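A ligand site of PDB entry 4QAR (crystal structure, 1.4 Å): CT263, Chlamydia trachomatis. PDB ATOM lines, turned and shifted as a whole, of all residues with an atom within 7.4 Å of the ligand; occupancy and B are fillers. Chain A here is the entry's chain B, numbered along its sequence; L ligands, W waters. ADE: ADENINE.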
ATOM      1  N   GLU A  18      31.328  -5.726 -12.342  1.00  0.00           N
ATOM      2  CA  GLU A  18      32.523  -6.550 -12.361  1.00  0.00           C
ATOM      3  C   GLU A  18      33.763  -5.689 -12.576  1.00  0.00           C
ATOM      4  O   GLU A  18      34.829  -5.987 -12.009  1.00  0.00           O
ATOM      5  CB  GLU A  18      32.376  -7.649 -13.403  1.00  0.00           C
ATOM      6  CG  GLU A  18      31.161  -8.533 -13.038  1.00  0.00           C
ATOM      7  CD  GLU A  18      30.898  -9.749 -13.915  1.00  0.00           C
ATOM      8  OE1 GLU A  18      31.807 -10.244 -14.590  1.00  0.00           O
ATOM      9  OE2 GLU A  18      29.734 -10.231 -13.907  1.00  0.00           O
ATOM     10  N   GLY A  76      36.234 -11.563 -15.100  1.00  0.00           N
ATOM     11  CA  GLY A  76      34.845 -11.515 -14.688  1.00  0.00           C
ATOM     12  C   GLY A  76      34.463 -12.558 -13.646  1.00  0.00           C
ATOM     13  O   GLY A  76      35.282 -13.375 -13.203  1.00  0.00           O
ATOM     14  N   PHE A  77      33.182 -12.509 -13.268  1.00  0.00           N
ATOM     15  CA  PHE A  77      32.605 -13.451 -12.319  1.00  0.00           C
ATOM     16  C   PHE A  77      32.243 -14.737 -13.071  1.00  0.00           C
ATOM     17  O   PHE A  77      31.786 -14.685 -14.224  1.00  0.00           O
ATOM     18  CB  PHE A  77      31.329 -12.880 -11.715  1.00  0.00           C
ATOM     19  CG  PHE A  77      31.471 -11.579 -10.955  1.00  0.00           C
ATOM     20  CD1 PHE A  77      32.706 -11.023 -10.663  1.00  0.00           C
ATOM     21  CD2 PHE A  77      30.345 -10.904 -10.523  1.00  0.00           C
ATOM     22  CE1 PHE A  77      32.788  -9.820  -9.946  1.00  0.00           C
ATOM     23  CE2 PHE A  77      30.427  -9.712  -9.786  1.00  0.00           C
ATOM     24  CZ  PHE A  77      31.660  -9.158  -9.517  1.00  0.00           C
ATOM     25  N   ALA A  78      32.444 -15.880 -12.424  1.00  0.00           N
ATOM     26  CA  ALA A  78      32.106 -17.168 -13.020  1.00  0.00           C
ATOM     27  C   ALA A  78      31.398 -18.047 -12.011  1.00  0.00           C
ATOM     28  O   ALA A  78      31.680 -17.997 -10.804  1.00  0.00           O
ATOM     29  CB  ALA A  78      33.354 -17.881 -13.569  1.00  0.00           C
ATOM     30  N   GLY A  79      30.501 -18.897 -12.507  1.00  0.00           N
ATOM     31  CA  GLY A  79      29.849 -19.854 -11.653  1.00  0.00           C
ATOM     32  C   GLY A  79      30.710 -21.078 -11.461  1.00  0.00           C
ATOM     33  O   GLY A  79      31.471 -21.462 -12.335  1.00  0.00           O
ATOM     34  N   ALA A  80      30.584 -21.694 -10.289  1.00  0.00           N
ATOM     35  CA  ALA A  80      31.307 -22.928  -9.986  1.00  0.00           C
ATOM     36  C   ALA A  80      30.339 -24.104 -10.119  1.00  0.00           C
ATOM     37  O   ALA A  80      29.330 -24.167  -9.406  1.00  0.00           O
ATOM     38  CB  ALA A  80      31.916 -22.888  -8.586  1.00  0.00           C
ATOM     39  N   THR A 123      33.691 -23.072 -19.264  1.00  0.00           N
ATOM     40  CA  THR A 123      32.622 -23.356 -20.216  1.00  0.00           C
ATOM     41  C   THR A 123      31.720 -22.138 -20.325  1.00  0.00           C
ATOM     42  O   THR A 123      31.236 -21.623 -19.313  1.00  0.00           O
ATOM     43  CB  THR A 123      31.831 -24.570 -19.755  1.00  0.00           C
ATOM     44  OG1 THR A 123      32.725 -25.670 -19.602  1.00  0.00           O
ATOM     45  CG2 THR A 123      30.739 -24.921 -20.759  1.00  0.00           C
ATOM     46  N   SER A 124      31.503 -21.664 -21.553  1.00  0.00           N
ATOM     47  CA  SER A 124      30.659 -20.511 -21.814  1.00  0.00           C
ATOM     48  C   SER A 124      29.288 -20.969 -22.291  1.00  0.00           C
ATOM     49  O   SER A 124      29.173 -21.823 -23.176  1.00  0.00           O
ATOM     50  CB  SER A 124      31.310 -19.612 -22.883  1.00  0.00           C
ATOM     51  OG  SER A 124      32.481 -18.999 -22.383  1.00  0.00           O
ATOM     52  N   VAL A 125      28.250 -20.397 -21.676  1.00  0.00           N
ATOM     53  CA  VAL A 125      26.868 -20.747 -21.922  1.00  0.00           C
ATOM     54  C   VAL A 125      26.109 -19.510 -22.376  1.00  0.00           C
ATOM     55  O   VAL A 125      26.565 -18.373 -22.213  1.00  0.00           O
ATOM     56  CB  VAL A 125      26.201 -21.354 -20.674  1.00  0.00           C
ATOM     57  CG1 VAL A 125      26.899 -22.639 -20.261  1.00  0.00           C
ATOM     58  CG2 VAL A 125      26.195 -20.388 -19.510  1.00  0.00           C
ATOM     59  N   ARG A 126      24.940 -19.746 -22.952  1.00  0.00           N
ATOM     60  CA  ARG A 126      24.092 -18.697 -23.493  1.00  0.00           C
ATOM     61  C   ARG A 126      22.889 -18.377 -22.603  1.00  0.00           C
ATOM     62  O   ARG A 126      22.000 -17.647 -23.027  1.00  0.00           O
ATOM     63  CB  ARG A 126      23.618 -19.079 -24.900  1.00  0.00           C
ATOM     64  N   SER A 127      22.854 -18.915 -21.384  1.00  0.00           N
ATOM     65  CA  SER A 127      21.828 -18.577 -20.397  1.00  0.00           C
ATOM     66  C   SER A 127      22.399 -18.883 -19.022  1.00  0.00           C
ATOM     67  O   SER A 127      23.302 -19.716 -18.908  1.00  0.00           O
ATOM     68  CB  SER A 127      20.552 -19.391 -20.635  1.00  0.00           C
ATOM     69  OG  SER A 127      20.159 -19.314 -21.997  1.00  0.00           O
ATOM     70  N   PRO A 128      21.912 -18.223 -17.963  1.00  0.00           N
ATOM     71  CA  PRO A 128      22.423 -18.528 -16.617  1.00  0.00           C
ATOM     72  C   PRO A 128      22.323 -20.020 -16.306  1.00  0.00           C
ATOM     73  O   PRO A 128      21.238 -20.604 -16.379  1.00  0.00           O
ATOM     74  CB  PRO A 128      21.518 -17.698 -15.695  1.00  0.00           C
ATOM     75  CG  PRO A 128      20.882 -16.664 -16.575  1.00  0.00           C
ATOM     76  CD  PRO A 128      20.778 -17.279 -17.940  1.00  0.00           C
ATOM     77  N   TYR A 129      23.447 -20.630 -15.975  1.00  0.00           N
ATOM     78  CA  TYR A 129      23.520 -22.070 -15.758  1.00  0.00           C
ATOM     79  C   TYR A 129      23.248 -22.362 -14.289  1.00  0.00           C
ATOM     80  O   TYR A 129      24.001 -21.937 -13.413  1.00  0.00           O
ATOM     81  CB  TYR A 129      24.894 -22.586 -16.190  1.00  0.00           C
ATOM     82  CG  TYR A 129      25.039 -24.072 -16.115  1.00  0.00           C
ATOM     83  CD1 TYR A 129      24.650 -24.895 -17.166  1.00  0.00           C
ATOM     84  CD2 TYR A 129      25.590 -24.681 -14.995  1.00  0.00           C
ATOM     85  CE1 TYR A 129      24.790 -26.264 -17.093  1.00  0.00           C
ATOM     86  CE2 TYR A 129      25.734 -26.052 -14.914  1.00  0.00           C
ATOM     87  CZ  TYR A 129      25.334 -26.844 -15.963  1.00  0.00           C
ATOM     88  OH  TYR A 129      25.473 -28.223 -15.871  1.00  0.00           O
ATOM     89  N   ARG A 130      22.146 -23.094 -14.035  1.00  0.00           N
ATOM     90  CA  ARG A 130      21.698 -23.462 -12.699  1.00  0.00           C
ATOM     91  C   ARG A 130      21.410 -24.958 -12.598  1.00  0.00           C
ATOM     92  O   ARG A 130      20.649 -25.376 -11.721  1.00  0.00           O
ATOM     93  CB  ARG A 130      20.429 -22.688 -12.315  1.00  0.00           C
ATOM     94  CG  ARG A 130      20.575 -21.189 -12.332  1.00  0.00           C
ATOM     95  CD  ARG A 130      21.391 -20.756 -11.146  1.00  0.00           C
ATOM     96  NE  ARG A 130      21.866 -19.392 -11.303  1.00  0.00           N
ATOM     97  CZ  ARG A 130      22.933 -18.907 -10.679  1.00  0.00           C
ATOM     98  NH1 ARG A 130      23.630 -19.670  -9.825  1.00  0.00           N
ATOM     99  NH2 ARG A 130      23.286 -17.655 -10.911  1.00  0.00           N
ATOM    100  N   VAL A 140      31.906 -21.641 -15.091  1.00  0.00           N
ATOM    101  CA  VAL A 140      30.923 -21.379 -16.125  1.00  0.00           C
ATOM    102  C   VAL A 140      30.712 -19.868 -16.232  1.00  0.00           C
ATOM    103  O   VAL A 140      30.518 -19.193 -15.216  1.00  0.00           O
ATOM    104  CB  VAL A 140      29.607 -22.149 -15.855  1.00  0.00           C
ATOM    105  CG1 VAL A 140      28.580 -21.809 -16.918  1.00  0.00           C
ATOM    106  CG2 VAL A 140      29.823 -23.666 -15.807  1.00  0.00           C
ATOM    107  N   ASP A 141      30.739 -19.336 -17.450  1.00  0.00           N
ATOM    108  CA  ASP A 141      30.477 -17.915 -17.702  1.00  0.00           C
ATOM    109  C   ASP A 141      29.653 -17.785 -18.980  1.00  0.00           C
ATOM    110  O   ASP A 141      29.118 -18.777 -19.487  1.00  0.00           O
ATOM    111  CB  ASP A 141      31.766 -17.113 -17.796  1.00  0.00           C
ATOM    112  CG  ASP A 141      32.428 -17.209 -19.181  1.00  0.00           C
ATOM    113  OD1 ASP A 141      32.177 -18.181 -19.926  1.00  0.00           O
ATOM    114  OD2 ASP A 141      33.221 -16.300 -19.517  1.00  0.00           O
ATOM    115  N   MET A 142      29.531 -16.556 -19.484  1.00  0.00           N
ATOM    116  CA  MET A 142      28.787 -16.288 -20.717  1.00  0.00           C
ATOM    117  C   MET A 142      29.568 -15.662 -21.853  1.00  0.00           C
ATOM    118  O   MET A 142      29.087 -15.704 -22.985  1.00  0.00           O
ATOM    119  CB  MET A 142      27.539 -15.446 -20.404  1.00  0.00           C
ATOM    120  CG  MET A 142      26.613 -16.119 -19.441  1.00  0.00           C
ATOM    121  SD  MET A 142      25.182 -15.126 -18.980  1.00  0.00           S
ATOM    122  CE  MET A 142      24.262 -16.282 -18.004  1.00  0.00           C
ATOM    123  N   GLU A 143      30.783 -15.124 -21.602  1.00  0.00           N
ATOM    124  CA  GLU A 143      31.503 -14.321 -22.601  1.00  0.00           C
ATOM    125  C   GLU A 143      32.818 -14.916 -23.061  1.00  0.00           C
ATOM    126  O   GLU A 143      33.239 -14.611 -24.167  1.00  0.00           O
ATOM    127  CB  GLU A 143      31.777 -12.904 -22.058  1.00  0.00           C
ATOM    128  CG  GLU A 143      30.558 -12.087 -21.763  1.00  0.00           C
ATOM    129  CD  GLU A 143      29.976 -12.385 -20.408  1.00  0.00           C
ATOM    130  OE1 GLU A 143      30.714 -12.914 -19.515  1.00  0.00           O
ATOM    131  OE2 GLU A 143      28.769 -12.123 -20.277  1.00  0.00           O
ATOM    132  N   VAL A 163      36.714 -15.199 -11.240  1.00  0.00           N
ATOM    133  CA  VAL A 163      36.572 -15.384  -9.800  1.00  0.00           C
ATOM    134  C   VAL A 163      35.271 -16.120  -9.573  1.00  0.00           C
ATOM    135  O   VAL A 163      34.227 -15.764 -10.123  1.00  0.00           O
ATOM    136  CB  VAL A 163      36.635 -14.049  -9.031  1.00  0.00           C
ATOM    137  CG1 VAL A 163      35.527 -13.075  -9.424  1.00  0.00           C
ATOM    138  CG2 VAL A 163      36.651 -14.273  -7.489  1.00  0.00           C
ATOM    139  N   SER A 164      35.339 -17.162  -8.744  1.00  0.00           N
ATOM    140  CA  SER A 164      34.160 -17.976  -8.488  1.00  0.00           C
ATOM    141  C   SER A 164      33.172 -17.177  -7.639  1.00  0.00           C
ATOM    142  O   SER A 164      33.498 -16.711  -6.527  1.00  0.00           O
ATOM    143  CB  SER A 164      34.578 -19.264  -7.812  1.00  0.00           C
ATOM    144  OG  SER A 164      35.415 -18.974  -6.704  1.00  0.00           O
ATOM    145  N   SER A 165      31.984 -16.963  -8.184  1.00  0.00           N
ATOM    146  CA  SER A 165      31.021 -15.986  -7.681  1.00  0.00           C
ATOM    147  C   SER A 165      29.713 -16.600  -7.221  1.00  0.00           C
ATOM    148  O   SER A 165      28.934 -15.905  -6.575  1.00  0.00           O
ATOM    149  CB  SER A 165      30.699 -14.947  -8.782  1.00  0.00           C
ATOM    150  OG  SER A 165      30.216 -15.547  -9.971  1.00  0.00           O
ATOM    151  N   ASP A 166      29.460 -17.855  -7.544  1.00  0.00           N
ATOM    152  CA  ASP A 166      28.218 -18.530  -7.182  1.00  0.00           C
ATOM    153  C   ASP A 166      28.387 -20.000  -7.526  1.00  0.00           C
ATOM    154  O   ASP A 166      29.162 -20.355  -8.410  1.00  0.00           O
ATOM    155  CB  ASP A 166      27.019 -17.963  -7.949  1.00  0.00           C
ATOM    156  CG  ASP A 166      27.193 -18.011  -9.460  1.00  0.00           C
ATOM    157  OD1 ASP A 166      27.951 -17.212 -10.009  1.00  0.00           O
ATOM    158  OD2 ASP A 166      26.561 -18.848 -10.132  1.00  0.00           O
ATOM    159  N   TYR A 167      27.611 -20.854  -6.849  1.00  0.00           N
ATOM    160  CA  TYR A 167      27.437 -22.224  -7.301  1.00  0.00           C
ATOM    161  C   TYR A 167      26.299 -22.265  -8.321  1.00  0.00           C
ATOM    162  O   TYR A 167      25.380 -21.450  -8.276  1.00  0.00           O
ATOM    163  CB  TYR A 167      27.179 -23.193  -6.138  1.00  0.00           C
ATOM    164  CG  TYR A 167      28.459 -23.436  -5.349  1.00  0.00           C
ATOM    165  CD1 TYR A 167      29.555 -24.057  -5.944  1.00  0.00           C
ATOM    166  CD2 TYR A 167      28.583 -23.016  -4.018  1.00  0.00           C
ATOM    167  CE1 TYR A 167      30.732 -24.225  -5.226  1.00  0.00           C
ATOM    168  CE2 TYR A 167      29.744 -23.170  -3.323  1.00  0.00           C
ATOM    169  CZ  TYR A 167      30.810 -23.797  -3.896  1.00  0.00           C
ATOM    170  OH  TYR A 167      31.990 -23.976  -3.204  1.00  0.00           O
ATOM    171  N   THR A 168      26.395 -23.204  -9.272  1.00  0.00           N
ATOM    172  CA  THR A 168      25.416 -23.308 -10.340  1.00  0.00           C
ATOM    173  C   THR A 168      24.202 -24.124  -9.903  1.00  0.00           C
ATOM    174  O   THR A 168      23.823 -25.083 -10.590  1.00  0.00           O
ATOM    175  CB  THR A 168      26.058 -23.965 -11.576  1.00  0.00           C
ATOM    176  OG1 THR A 168      26.580 -25.265 -11.237  1.00  0.00           O
ATOM    177  CG2 THR A 168      27.188 -23.119 -12.104  1.00  0.00           C
ATOM    178  N   THR A 169      23.671 -23.796  -8.729  1.00  0.00           N
ATOM    179  CA  THR A 169      22.422 -24.298  -8.177  1.00  0.00           C
ATOM    180  C   THR A 169      21.417 -23.156  -8.083  1.00  0.00           C
ATOM    181  O   THR A 169      21.753 -21.975  -8.180  1.00  0.00           O
ATOM    182  CB  THR A 169      22.683 -24.914  -6.802  1.00  0.00           C
ATOM    183  OG1 THR A 169      23.488 -24.033  -6.014  1.00  0.00           O
ATOM    184  CG2 THR A 169      23.425 -26.224  -6.926  1.00  0.00           C
ATOM    185  N   GLY A 172      21.644 -19.490  -6.555  1.00  0.00           N
ATOM    186  CA  GLY A 172      23.062 -19.300  -6.263  1.00  0.00           C
ATOM    187  C   GLY A 172      23.546 -17.893  -6.514  1.00  0.00           C
ATOM    188  O   GLY A 172      24.571 -17.469  -5.953  1.00  0.00           O
ATOM    189  N   GLN A 173      22.811 -17.137  -7.330  1.00  0.00           N
ATOM    190  CA  GLN A 173      23.175 -15.749  -7.601  1.00  0.00           C
ATOM    191  C   GLN A 173      23.099 -14.896  -6.345  1.00  0.00           C
ATOM    192  O   GLN A 173      23.652 -13.802  -6.322  1.00  0.00           O
ATOM    193  CB  GLN A 173      22.269 -15.149  -8.694  1.00  0.00           C
ATOM    194  CG  GLN A 173      20.754 -15.080  -8.358  1.00  0.00           C
ATOM    195  CD  GLN A 173      19.925 -16.323  -8.756  1.00  0.00           C
ATOM    196  OE1 GLN A 173      20.391 -17.450  -8.685  1.00  0.00           O
ATOM    197  NE2 GLN A 173      18.671 -16.110  -9.186  1.00  0.00           N
ATOM    198  N   LEU A 176      26.564 -14.107  -5.261  1.00  0.00           N
ATOM    199  CA  LEU A 176      27.172 -13.118  -6.134  1.00  0.00           C
ATOM    200  C   LEU A 176      26.657 -11.708  -5.803  1.00  0.00           C
ATOM    201  O   LEU A 176      27.436 -10.769  -5.624  1.00  0.00           O
ATOM    202  CB  LEU A 176      26.874 -13.501  -7.583  1.00  0.00           C
ATOM    203  CG  LEU A 176      27.434 -12.659  -8.738  1.00  0.00           C
ATOM    204  CD1 LEU A 176      27.317 -13.435  -9.993  1.00  0.00           C
ATOM    205  CD2 LEU A 176      26.699 -11.348  -8.928  1.00  0.00           C
HETATM  206  N9  ADE L   1      28.574 -16.053 -14.477  1.00  0.00           N
HETATM  207  C8  ADE L   1      28.553 -16.072 -13.114  1.00  0.00           C
HETATM  208  N7  ADE L   1      27.820 -17.027 -12.614  1.00  0.00           N
HETATM  209  C5  ADE L   1      27.332 -17.697 -13.730  1.00  0.00           C
HETATM  210  C6  ADE L   1      26.497 -18.815 -13.873  1.00  0.00           C
HETATM  211  N6  ADE L   1      26.000 -19.495 -12.837  1.00  0.00           N
HETATM  212  N1  ADE L   1      26.189 -19.215 -15.132  1.00  0.00           N
HETATM  213  C2  ADE L   1      26.693 -18.529 -16.169  1.00  0.00           C
HETATM  214  N3  ADE L   1      27.489 -17.461 -16.155  1.00  0.00           N
HETATM  215  C4  ADE L   1      27.781 -17.104 -14.888  1.00  0.00           C
HETATM  216  O   HOH W   1      28.626 -12.723 -14.082  1.00  0.00           O
HETATM  217  O   HOH W   2      29.530 -14.643 -17.354  1.00  0.00           O
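The side-chain carboxylate of Asp 166 is in hydrogen-bond range of a nitrogen (N7) of the ligand.
N of Tyr 129 is in hydrogen-bond range of N1 of the ligand (3.2 Å).
O of Tyr 129 lies within hydrogen-bond range of N6 of the ligand, 3.2 Å away.
N7 of the ligand lies within hydrogen-bond range of N of Gly 79 (3.3 Å).
The side-chain carboxylate of Asp 166 sits at hydrogen-bond distance from the side-chain hydroxyl of Ser 165.
OD2 of Asp 166 lies within salt-bridge range of NH1 of Arg 130.
OD2 of Asp 141 sits at hydrogen-bond distance from N of Glu 143.
N of Asp 141 lies within hydrogen-bond range of O of Thr 123, at 3.0 Å.
OG of Ser 124 lies within hydrogen-bond range of OD1 of Asp 141, at 2.6 Å.
The backbone NH (N) of Phe 77 is in hydrogen-bond range of the side-chain carboxylate (OE1) of Glu 18 (3.0 Å).
The backbone carbonyl oxygen (O) of Thr 169 sits close to the guanidinium group (NH1) of Arg 130, at 3.4 Å.
N of Thr 168 is in hydrogen-bond range of O of Ala 80 (3.1 Å).
Phe 77 touches the ligand (O to N9, 3.5 Å).
Ala 78 touches the ligand.
CG2 of Val 125 touches C2 of the ligand (3.9 Å).
Arg 130 touches the ligand.
Val 140 touches the ligand (O to C4, 3.5 Å).
CA of Asp 141 touches N3 of the ligand, at 3.4 Å.
CG of Met 142 touches N3 of the ligand, at 3.7 Å.
OG of Ser 165 touches C8 of the ligand, 3.6 Å away.
CG2 of Thr 168 touches N6 of the ligand (3.9 Å).
Hydrophobic or aromatic side chains within 4 Å of the ligand: Val 125, Tyr 129, Val 140 and Met 142.
12 residues have an atom within 4 Å of the ligand: Phe 77, Ala 78, Gly 79, Val 125, Tyr 129, Arg 130, Val 140, Asp 141, Met 142, Ser 165, Asp 166 and Thr 168.
The nearest printed residue that does not touch the ligand is Pro 128 (4.1 Å).
Water W2 lies within hydrogen-bond range of N of Met 142 (2.9 Å), OE1 of Glu 143 (3.0 Å) and N9 of the ligand (3.3 Å).
Water W1 bridges the side-chain carboxylate (OE2) of Glu 18 (2.7 Å) and a nitrogen (N9) of the ligand (3.4 Å).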
